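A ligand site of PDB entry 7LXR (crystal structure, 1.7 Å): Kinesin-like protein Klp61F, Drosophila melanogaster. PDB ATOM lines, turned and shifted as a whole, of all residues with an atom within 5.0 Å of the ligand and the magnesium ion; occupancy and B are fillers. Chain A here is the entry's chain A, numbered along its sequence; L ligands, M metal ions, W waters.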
ATOM      1  N   ARG A  27      20.074  18.287  -0.723  1.00  0.00           N
ATOM      2  CA  ARG A  27      19.805  16.933  -0.205  1.00  0.00           C
ATOM      3  C   ARG A  27      19.250  17.027   1.183  1.00  0.00           C
ATOM      4  O   ARG A  27      19.901  17.658   2.077  1.00  0.00           O
ATOM      5  CB  ARG A  27      21.043  16.023  -0.214  1.00  0.00           C
ATOM      6  CG  ARG A  27      20.673  14.587   0.169  1.00  0.00           C
ATOM      7  CD  ARG A  27      21.860  13.635   0.167  1.00  0.00           C
ATOM      8  NE  ARG A  27      21.388  12.269   0.221  1.00  0.00           N
ATOM      9  CZ  ARG A  27      22.134  11.206   0.162  1.00  0.00           C
ATOM     10  NH1 ARG A  27      23.429  11.322   0.159  1.00  0.00           N
ATOM     11  NH2 ARG A  27      21.579  10.026  -0.007  1.00  0.00           N
ATOM     12  N   ARG A  29      18.077  15.139   4.452  1.00  0.00           N
ATOM     13  CA  ARG A  29      18.278  13.854   5.154  1.00  0.00           C
ATOM     14  C   ARG A  29      16.921  13.444   5.743  1.00  0.00           C
ATOM     15  O   ARG A  29      16.063  14.280   6.044  1.00  0.00           O
ATOM     16  CB  ARG A  29      19.368  13.946   6.224  1.00  0.00           C
ATOM     17  CG  ARG A  29      19.006  14.846   7.409  1.00  0.00           C
ATOM     18  CD  ARG A  29      19.731  14.308   8.627  1.00  0.00           C
ATOM     19  NE  ARG A  29      19.772  15.232   9.740  1.00  0.00           N
ATOM     20  CZ  ARG A  29      18.792  15.324  10.627  1.00  0.00           C
ATOM     21  NH1 ARG A  29      17.682  14.641  10.433  1.00  0.00           N
ATOM     22  NH2 ARG A  29      18.914  16.081  11.696  1.00  0.00           N
ATOM     23  N   PRO A  30      16.739  12.133   6.017  1.00  0.00           N
ATOM     24  CA  PRO A  30      15.589  11.694   6.797  1.00  0.00           C
ATOM     25  C   PRO A  30      15.658  12.191   8.247  1.00  0.00           C
ATOM     26  O   PRO A  30      16.752  12.458   8.786  1.00  0.00           O
ATOM     27  CB  PRO A  30      15.622  10.158   6.775  1.00  0.00           C
ATOM     28  CG  PRO A  30      16.881   9.786   6.055  1.00  0.00           C
ATOM     29  CD  PRO A  30      17.618  11.031   5.617  1.00  0.00           C
ATOM     30  N   PRO A  74      14.432  12.633   1.322  1.00  0.00           N
ATOM     31  CA  PRO A  74      14.938  11.692   2.338  1.00  0.00           C
ATOM     32  C   PRO A  74      15.083  10.222   1.918  1.00  0.00           C
ATOM     33  O   PRO A  74      15.880   9.535   2.540  1.00  0.00           O
ATOM     34  CB  PRO A  74      13.968  11.900   3.523  1.00  0.00           C
ATOM     35  CG  PRO A  74      12.756  12.599   2.939  1.00  0.00           C
ATOM     36  CD  PRO A  74      13.215  13.355   1.706  1.00  0.00           C
ATOM     37  N   GLY A 105      26.430  22.830   4.773  1.00  0.00           N
ATOM     38  CA  GLY A 105      25.145  22.821   5.512  1.00  0.00           C
ATOM     39  C   GLY A 105      25.301  22.714   7.015  1.00  0.00           C
ATOM     40  O   GLY A 105      26.412  22.508   7.519  1.00  0.00           O
ATOM     41  N   GLN A 106      24.180  22.790   7.737  1.00  0.00           N
ATOM     42  CA  GLN A 106      24.171  22.672   9.210  1.00  0.00           C
ATOM     43  C   GLN A 106      24.849  21.365   9.673  1.00  0.00           C
ATOM     44  O   GLN A 106      24.798  20.342   8.960  1.00  0.00           O
ATOM     45  CB  GLN A 106      22.733  22.828   9.666  1.00  0.00           C
ATOM     46  CG  GLN A 106      22.546  22.726  11.171  1.00  0.00           C
ATOM     47  CD  GLN A 106      21.071  22.670  11.493  1.00  0.00           C
ATOM     48  OE1 GLN A 106      20.227  22.367  10.674  1.00  0.00           O
ATOM     49  NE2 GLN A 106      20.753  23.086  12.716  1.00  0.00           N
ATOM     50  N   THR A 107      25.451  21.416  10.863  1.00  0.00           N
ATOM     51  CA  THR A 107      25.938  20.182  11.542  1.00  0.00           C
ATOM     52  C   THR A 107      24.853  19.082  11.491  1.00  0.00           C
ATOM     53  O   THR A 107      23.629  19.325  11.779  1.00  0.00           O
ATOM     54  CB  THR A 107      26.468  20.522  12.936  1.00  0.00           C
ATOM     55  OG1 THR A 107      27.018  19.333  13.494  1.00  0.00           O
ATOM     56  CG2 THR A 107      25.382  20.997  13.866  1.00  0.00           C
ATOM     57  N   GLY A 108      25.270  17.868  11.177  1.00  0.00           N
ATOM     58  CA  GLY A 108      24.429  16.665  11.305  1.00  0.00           C
ATOM     59  C   GLY A 108      23.466  16.500  10.149  1.00  0.00           C
ATOM     60  O   GLY A 108      22.594  15.656  10.270  1.00  0.00           O
ATOM     61  N   THR A 109      23.607  17.227   9.001  1.00  0.00           N
ATOM     62  CA  THR A 109      22.585  17.156   7.954  1.00  0.00           C
ATOM     63  C   THR A 109      22.980  16.184   6.836  1.00  0.00           C
ATOM     64  O   THR A 109      22.133  16.010   5.999  1.00  0.00           O
ATOM     65  CB  THR A 109      22.233  18.537   7.386  1.00  0.00           C
ATOM     66  OG1 THR A 109      23.490  19.099   6.986  1.00  0.00           O
ATOM     67  CG2 THR A 109      21.537  19.342   8.473  1.00  0.00           C
ATOM     68  N   GLY A 110      24.203  15.652   6.817  1.00  0.00           N
ATOM     69  CA  GLY A 110      24.528  14.564   5.910  1.00  0.00           C
ATOM     70  C   GLY A 110      25.628  14.872   4.957  1.00  0.00           C
ATOM     71  O   GLY A 110      25.747  14.125   3.972  1.00  0.00           O
ATOM     72  N   LYS A 111      26.507  15.844   5.296  1.00  0.00           N
ATOM     73  CA  LYS A 111      27.634  16.148   4.421  1.00  0.00           C
ATOM     74  C   LYS A 111      28.606  14.993   4.275  1.00  0.00           C
ATOM     75  O   LYS A 111      28.926  14.658   3.098  1.00  0.00           O
ATOM     76  CB  LYS A 111      28.351  17.417   4.880  1.00  0.00           C
ATOM     77  CG  LYS A 111      27.543  18.699   4.710  1.00  0.00           C
ATOM     78  CD  LYS A 111      28.184  19.905   5.345  1.00  0.00           C
ATOM     79  CE  LYS A 111      28.591  19.745   6.834  1.00  0.00           C
ATOM     80  NZ  LYS A 111      27.371  19.606   7.739  1.00  0.00           N
ATOM     81  N   THR A 112      29.034  14.413   5.386  1.00  0.00           N
ATOM     82  CA  THR A 112      30.080  13.358   5.346  1.00  0.00           C
ATOM     83  C   THR A 112      29.446  12.070   4.801  1.00  0.00           C
ATOM     84  O   THR A 112      30.078  11.413   3.968  1.00  0.00           O
ATOM     85  CB  THR A 112      30.697  13.193   6.701  1.00  0.00           C
ATOM     86  OG1 THR A 112      31.279  14.469   7.035  1.00  0.00           O
ATOM     87  CG2 THR A 112      31.706  12.069   6.772  1.00  0.00           C
ATOM     88  N   HIS A 113      28.212  11.811   5.166  1.00  0.00           N
ATOM     89  CA  HIS A 113      27.453  10.677   4.589  1.00  0.00           C
ATOM     90  C   HIS A 113      27.527  10.771   3.081  1.00  0.00           C
ATOM     91  O   HIS A 113      27.772   9.759   2.351  1.00  0.00           O
ATOM     92  CB  HIS A 113      26.036  10.687   5.122  1.00  0.00           C
ATOM     93  CG  HIS A 113      25.238   9.641   4.455  1.00  0.00           C
ATOM     94  ND1 HIS A 113      25.407   8.271   4.798  1.00  0.00           N
ATOM     95  CD2 HIS A 113      24.300   9.710   3.515  1.00  0.00           C
ATOM     96  CE1 HIS A 113      24.602   7.583   4.003  1.00  0.00           C
ATOM     97  NE2 HIS A 113      23.911   8.415   3.207  1.00  0.00           N
ATOM     98  N   THR A 114      27.198  11.958   2.568  1.00  0.00           N
ATOM     99  CA  THR A 114      27.097  12.227   1.119  1.00  0.00           C
ATOM    100  C   THR A 114      28.501  12.156   0.481  1.00  0.00           C
ATOM    101  O   THR A 114      28.658  11.482  -0.586  1.00  0.00           O
ATOM    102  CB  THR A 114      26.413  13.566   0.845  1.00  0.00           C
ATOM    103  OG1 THR A 114      25.101  13.483   1.359  1.00  0.00           O
ATOM    104  CG2 THR A 114      26.423  13.874  -0.641  1.00  0.00           C
ATOM    105  N   MET A 226      23.425  11.636  17.607  1.00  0.00           N
ATOM    106  CA  MET A 226      22.860  11.589  16.208  1.00  0.00           C
ATOM    107  C   MET A 226      23.876  12.087  15.188  1.00  0.00           C
ATOM    108  O   MET A 226      23.448  12.377  14.053  1.00  0.00           O
ATOM    109  CB  MET A 226      21.569  12.419  16.044  1.00  0.00           C
ATOM    110  CG  MET A 226      20.432  11.916  16.940  1.00  0.00           C
ATOM    111  SD  MET A 226      19.732  10.336  16.438  1.00  0.00           S
ATOM    112  CE  MET A 226      20.652   9.248  17.520  1.00  0.00           C
ATOM    113  N   ASN A 227      25.154  12.195  15.550  1.00  0.00           N
ATOM    114  CA  ASN A 227      26.212  12.815  14.698  1.00  0.00           C
ATOM    115  C   ASN A 227      27.535  12.271  15.228  1.00  0.00           C
ATOM    116  O   ASN A 227      28.377  13.058  15.694  1.00  0.00           O
ATOM    117  CB  ASN A 227      25.999  14.341  14.619  1.00  0.00           C
ATOM    118  CG  ASN A 227      26.903  15.041  13.624  1.00  0.00           C
ATOM    119  OD1 ASN A 227      27.460  14.410  12.689  1.00  0.00           O
ATOM    120  ND2 ASN A 227      27.050  16.335  13.854  1.00  0.00           N
ATOM    121  N   GLN A 229      30.143  10.829  14.125  1.00  0.00           N
ATOM    122  CA  GLN A 229      31.448  11.155  13.514  1.00  0.00           C
ATOM    123  C   GLN A 229      31.372  12.602  13.000  1.00  0.00           C
ATOM    124  O   GLN A 229      31.848  12.801  11.872  1.00  0.00           O
ATOM    125  CB  GLN A 229      31.802  10.177  12.376  1.00  0.00           C
ATOM    126  CG  GLN A 229      32.256   8.836  12.921  1.00  0.00           C
ATOM    127  CD  GLN A 229      31.937   7.713  11.987  1.00  0.00           C
ATOM    128  OE1 GLN A 229      31.155   6.821  12.341  1.00  0.00           O
ATOM    129  NE2 GLN A 229      32.527   7.772  10.790  1.00  0.00           N
ATOM    130  N   SER A 230      30.835  13.527  13.829  1.00  0.00           N
ATOM    131  CA  SER A 230      30.788  14.990  13.498  1.00  0.00           C
ATOM    132  C   SER A 230      32.162  15.440  13.009  1.00  0.00           C
ATOM    133  O   SER A 230      33.185  15.225  13.731  1.00  0.00           O
ATOM    134  CB  SER A 230      30.428  15.803  14.680  1.00  0.00           C
ATOM    135  OG  SER A 230      30.456  17.225  14.388  1.00  0.00           O
ATOM    136  N   SER A 231      32.230  16.088  11.860  1.00  0.00           N
ATOM    137  CA  SER A 231      33.464  16.660  11.295  1.00  0.00           C
ATOM    138  C   SER A 231      33.832  17.949  12.047  1.00  0.00           C
ATOM    139  O   SER A 231      33.050  18.922  11.998  1.00  0.00           O
ATOM    140  CB  SER A 231      33.288  16.891   9.825  1.00  0.00           C
ATOM    141  OG  SER A 231      32.733  15.753   9.192  1.00  0.00           O
ATOM    142  N   ASP A 263      34.502  18.118   1.840  1.00  0.00           N
ATOM    143  CA  ASP A 263      33.508  17.904   2.899  1.00  0.00           C
ATOM    144  C   ASP A 263      33.684  19.042   3.906  1.00  0.00           C
ATOM    145  O   ASP A 263      34.636  18.957   4.691  1.00  0.00           O
ATOM    146  CB  ASP A 263      33.788  16.545   3.552  1.00  0.00           C
ATOM    147  CG  ASP A 263      32.724  16.103   4.537  1.00  0.00           C
ATOM    148  OD1 ASP A 263      31.726  16.789   4.649  1.00  0.00           O
ATOM    149  OD2 ASP A 263      32.897  15.046   5.236  1.00  0.00           O
ATOM    150  N   LEU A 264      32.768  19.968   3.996  1.00  0.00           N
ATOM    151  CA  LEU A 264      32.903  21.058   4.990  1.00  0.00           C
ATOM    152  C   LEU A 264      32.400  20.544   6.362  1.00  0.00           C
ATOM    153  O   LEU A 264      31.391  19.770   6.392  1.00  0.00           O
ATOM    154  CB  LEU A 264      32.160  22.297   4.532  1.00  0.00           C
ATOM    155  CG  LEU A 264      32.618  22.916   3.211  1.00  0.00           C
ATOM    156  CD1 LEU A 264      31.793  24.121   2.938  1.00  0.00           C
ATOM    157  CD2 LEU A 264      34.090  23.191   3.216  1.00  0.00           C
ATOM    158  N   ALA A 265      32.953  21.076   7.436  1.00  0.00           N
ATOM    159  CA  ALA A 265      32.311  21.016   8.785  1.00  0.00           C
ATOM    160  C   ALA A 265      31.033  21.840   8.778  1.00  0.00           C
ATOM    161  O   ALA A 265      30.950  22.761   7.981  1.00  0.00           O
ATOM    162  CB  ALA A 265      33.226  21.545   9.827  1.00  0.00           C
ATOM    163  N   GLY A 266      30.052  21.519   9.615  1.00  0.00           N
ATOM    164  CA  GLY A 266      28.688  22.070   9.607  1.00  0.00           C
ATOM    165  C   GLY A 266      28.568  23.286  10.519  1.00  0.00           C
ATOM    166  O   GLY A 266      29.262  23.340  11.534  1.00  0.00           O
ATOM    167  N   THR A 334      23.101  20.558   2.165  1.00  0.00           N
ATOM    168  CA  THR A 334      22.422  19.502   2.968  1.00  0.00           C
ATOM    169  C   THR A 334      21.563  20.197   3.988  1.00  0.00           C
ATOM    170  O   THR A 334      22.073  21.192   4.628  1.00  0.00           O
ATOM    171  CB  THR A 334      23.418  18.535   3.638  1.00  0.00           C
ATOM    172  OG1 THR A 334      24.370  19.289   4.405  1.00  0.00           O
ATOM    173  CG2 THR A 334      24.245  17.803   2.624  1.00  0.00           C
HETATM  174  P1  LIG L   1      28.961  17.622  10.626  1.00  0.00           P
HETATM  175  O1  LIG L   1      29.052  17.725  12.123  1.00  0.00           O
HETATM  176  O2  LIG L   1      30.248  17.082  10.143  1.00  0.00           O
HETATM  177  O3  LIG L   1      28.637  18.959  10.006  1.00  0.00           O
HETATM  178  P2  LIG L   1      27.508  15.960   8.736  1.00  0.00           P
HETATM  179  O4  LIG L   1      28.811  15.559   8.097  1.00  0.00           O
HETATM  180  O5  LIG L   1      26.639  16.926   7.969  1.00  0.00           O
HETATM  181  N1  LIG L   1      27.818  16.533  10.218  1.00  0.00           N
HETATM  182  P3  LIG L   1      26.891  13.129   8.713  1.00  0.00           P
HETATM  183  O6  LIG L   1      28.039  12.644   9.483  1.00  0.00           O
HETATM  184  O7  LIG L   1      26.887  12.968   7.214  1.00  0.00           O
HETATM  185  O8  LIG L   1      26.646  14.657   9.100  1.00  0.00           O
HETATM  186  O9  LIG L   1      25.506  12.520   9.188  1.00  0.00           O
HETATM  187  C1  LIG L   1      25.023  12.607  10.540  1.00  0.00           C
HETATM  188  C2  LIG L   1      24.266  11.319  10.813  1.00  0.00           C
HETATM  189  O10 LIG L   1      23.077  11.270   9.990  1.00  0.00           O
HETATM  190  C3  LIG L   1      25.069  10.054  10.502  1.00  0.00           C
HETATM  191  O11 LIG L   1      24.816   9.026  11.445  1.00  0.00           O
HETATM  192  C4  LIG L   1      24.530   9.635   9.140  1.00  0.00           C
HETATM  193  O12 LIG L   1      24.609   8.237   8.954  1.00  0.00           O
HETATM  194  C5  LIG L   1      23.087  10.106   9.195  1.00  0.00           C
HETATM  195  N2  LIG L   1      22.638  10.432   7.877  1.00  0.00           N
HETATM  196  C6  LIG L   1      22.966  11.544   7.141  1.00  0.00           C
HETATM  197  N3  LIG L   1      22.397  11.568   5.961  1.00  0.00           N
HETATM  198  C7  LIG L   1      21.660  10.399   5.910  1.00  0.00           C
HETATM  199  C8  LIG L   1      20.829   9.837   4.898  1.00  0.00           C
HETATM  200  N4  LIG L   1      20.631  10.389   3.719  1.00  0.00           N
HETATM  201  N5  LIG L   1      20.231   8.651   5.166  1.00  0.00           N
HETATM  202  C9  LIG L   1      20.474   8.092   6.366  1.00  0.00           C
HETATM  203  N6  LIG L   1      21.250   8.505   7.371  1.00  0.00           N
HETATM  204  C10 LIG L   1      21.793   9.696   7.082  1.00  0.00           C
HETATM  205 MG    MG M   1      30.654  15.761   8.587  1.00  0.00          MG
HETATM  206  O   HOH W   1      20.655  12.033  11.103  1.00  0.00           O
HETATM  207  O   HOH W   2      30.886  20.042  12.447  1.00  0.00           O
HETATM  208  O   HOH W   3      30.280  14.101   9.794  1.00  0.00           O
HETATM  209  O   HOH W   4      18.806  12.182   1.701  1.00  0.00           O
HETATM  210  O   HOH W   5      18.443   9.543   1.894  1.00  0.00           O
HETATM  211  O   HOH W   6      22.213  12.863   3.336  1.00  0.00           O
HETATM  212  O   HOH W   7      28.269  11.812  12.107  1.00  0.00           O
HETATM  213  O   HOH W   8      25.684   9.101  13.953  1.00  0.00           O
HETATM  214  O   HOH W   9      29.324  10.235   8.868  1.00  0.00           O
HETATM  215  O   HOH W  10      20.859   7.109   9.827  1.00  0.00           O
HETATM  216  O   HOH W  11      31.029  17.285   7.192  1.00  0.00           O
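The side-chain hydroxyl (OG1) of Thr 112 lies close to the side-chain carboxylate (OD2) of Asp 263, 2.5 Å away. The backbone carbonyl oxygen of Gln 106 sits at hydrogen-bond distance from the side-chain amino group of Lys 111. The side-chain amino group (NZ) of Lys 111 sits at hydrogen-bond distance from the backbone carbonyl oxygen (O) of Gly 105 (3.1 Å). ND2 of Asn 227 sits at hydrogen-bond distance from OG1 of Thr 107 (3.0 Å). O of Gly 110 sits at hydrogen-bond distance from OG1 of Thr 114 (2.8 Å). O of Gly 108 is in hydrogen-bond range of NE of Arg 29, 2.9 Å away. The side-chain hydroxyl of Thr 334 is in hydrogen-bond range of the side-chain hydroxyl of Thr 109 (2.7 Å). The side-chain hydroxyl (OG1) of Thr 114 sits at hydrogen-bond distance from the guanidinium group (NH1) of Arg 27 (3.0 Å).
A nitrogen (N1) of the ligand sits close to the backbone NH (N) of Gly 108, at 3.0 Å. NH2 of Arg 27 touches N4 of the ligand, at 3.9 Å. CB of Arg 29 touches N3 of the ligand, at 3.9 Å. Pro 30 touches the ligand. Met 226 touches the ligand (O to C2, 3.5 Å). C of Ala 265 touches O3 of the ligand, at 3.9 Å. Hydrophobic or aromatic side chains within 4 Å of the ligand: Pro 30 and His 113. Of the 24 residues printed, 16 come within 4 Å of the ligand.
The magnesium ion is bound by O4 of the ligand (1.9 Å), O2 of the ligand (2.1 Å), water W3 (2.1 Å), water W11 (2.1 Å), OG1 of Thr 112 (2.1 Å) and OG of Ser 231 (2.2 Å).
Of the 24 residues printed, 2 come within 4 Å of the magnesium ion. The nearest printed residue that does not touch the magnesium ion is Asp 263 (4.1 Å).
N of Thr 112 is in hydrogen-bond range of O7 of the ligand (3.2 Å). An oxygen (O2) of the ligand lies close to the backbone NH (N) of Ser 231 (2.8 Å). O5 of the ligand sits at hydrogen-bond distance from N of Lys 111, at 2.9 Å. An oxygen (O3) of the ligand is in salt-bridge range of the side-chain amino group of Lys 111, at 2.7 Å. An oxygen (O7) of the ligand is in hydrogen-bond range of the backbone NH (N) of His 113 (2.7 Å). OG of Ser 230 is in hydrogen-bond range of O1 of the ligand (2.7 Å). OG1 of Thr 107 sits at hydrogen-bond distance from O1 of the ligand (2.9 Å). An oxygen (O3) of the ligand is in hydrogen-bond range of the backbone NH (N) of Gly 266, 3.0 Å away. The backbone NH (N) of Gly 110 lies within hydrogen-bond range of an oxygen (O5) of the ligand. An oxygen (O1) of the ligand sits at hydrogen-bond distance from the side-chain amide nitrogen of Asn 227, 3.0 Å away. N of Thr 109 is in hydrogen-bond range of O5 of the ligand (3.2 Å).
Water W3 lies within hydrogen-bond range of O6 of the ligand (2.7 Å), O of Gln 229 (2.9 Å) and N of Ser 231 (3.5 Å). Water W11 bridges O of Leu 264 (2.6 Å) and OD1 of Asp 263 (2.7 Å). Water W7 lies within hydrogen-bond range of O6 of the ligand, OD1 of Asn 227 and N of Gln 229. Water W6 lies within hydrogen-bond range of a nitrogen (N3) of the ligand and the guanidinium group of Arg 27. Water W2 lies within hydrogen-bond range of the backbone carbonyl oxygen of Ser 231 (2.5 Å), an oxygen (O1) of the ligand (3.0 Å), the backbone NH of Gly 266 (3.3 Å) and the side-chain hydroxyl of Ser 230 (3.4 Å). Water W4 lies within hydrogen-bond range of NE of Arg 27 and N4 of the ligand.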
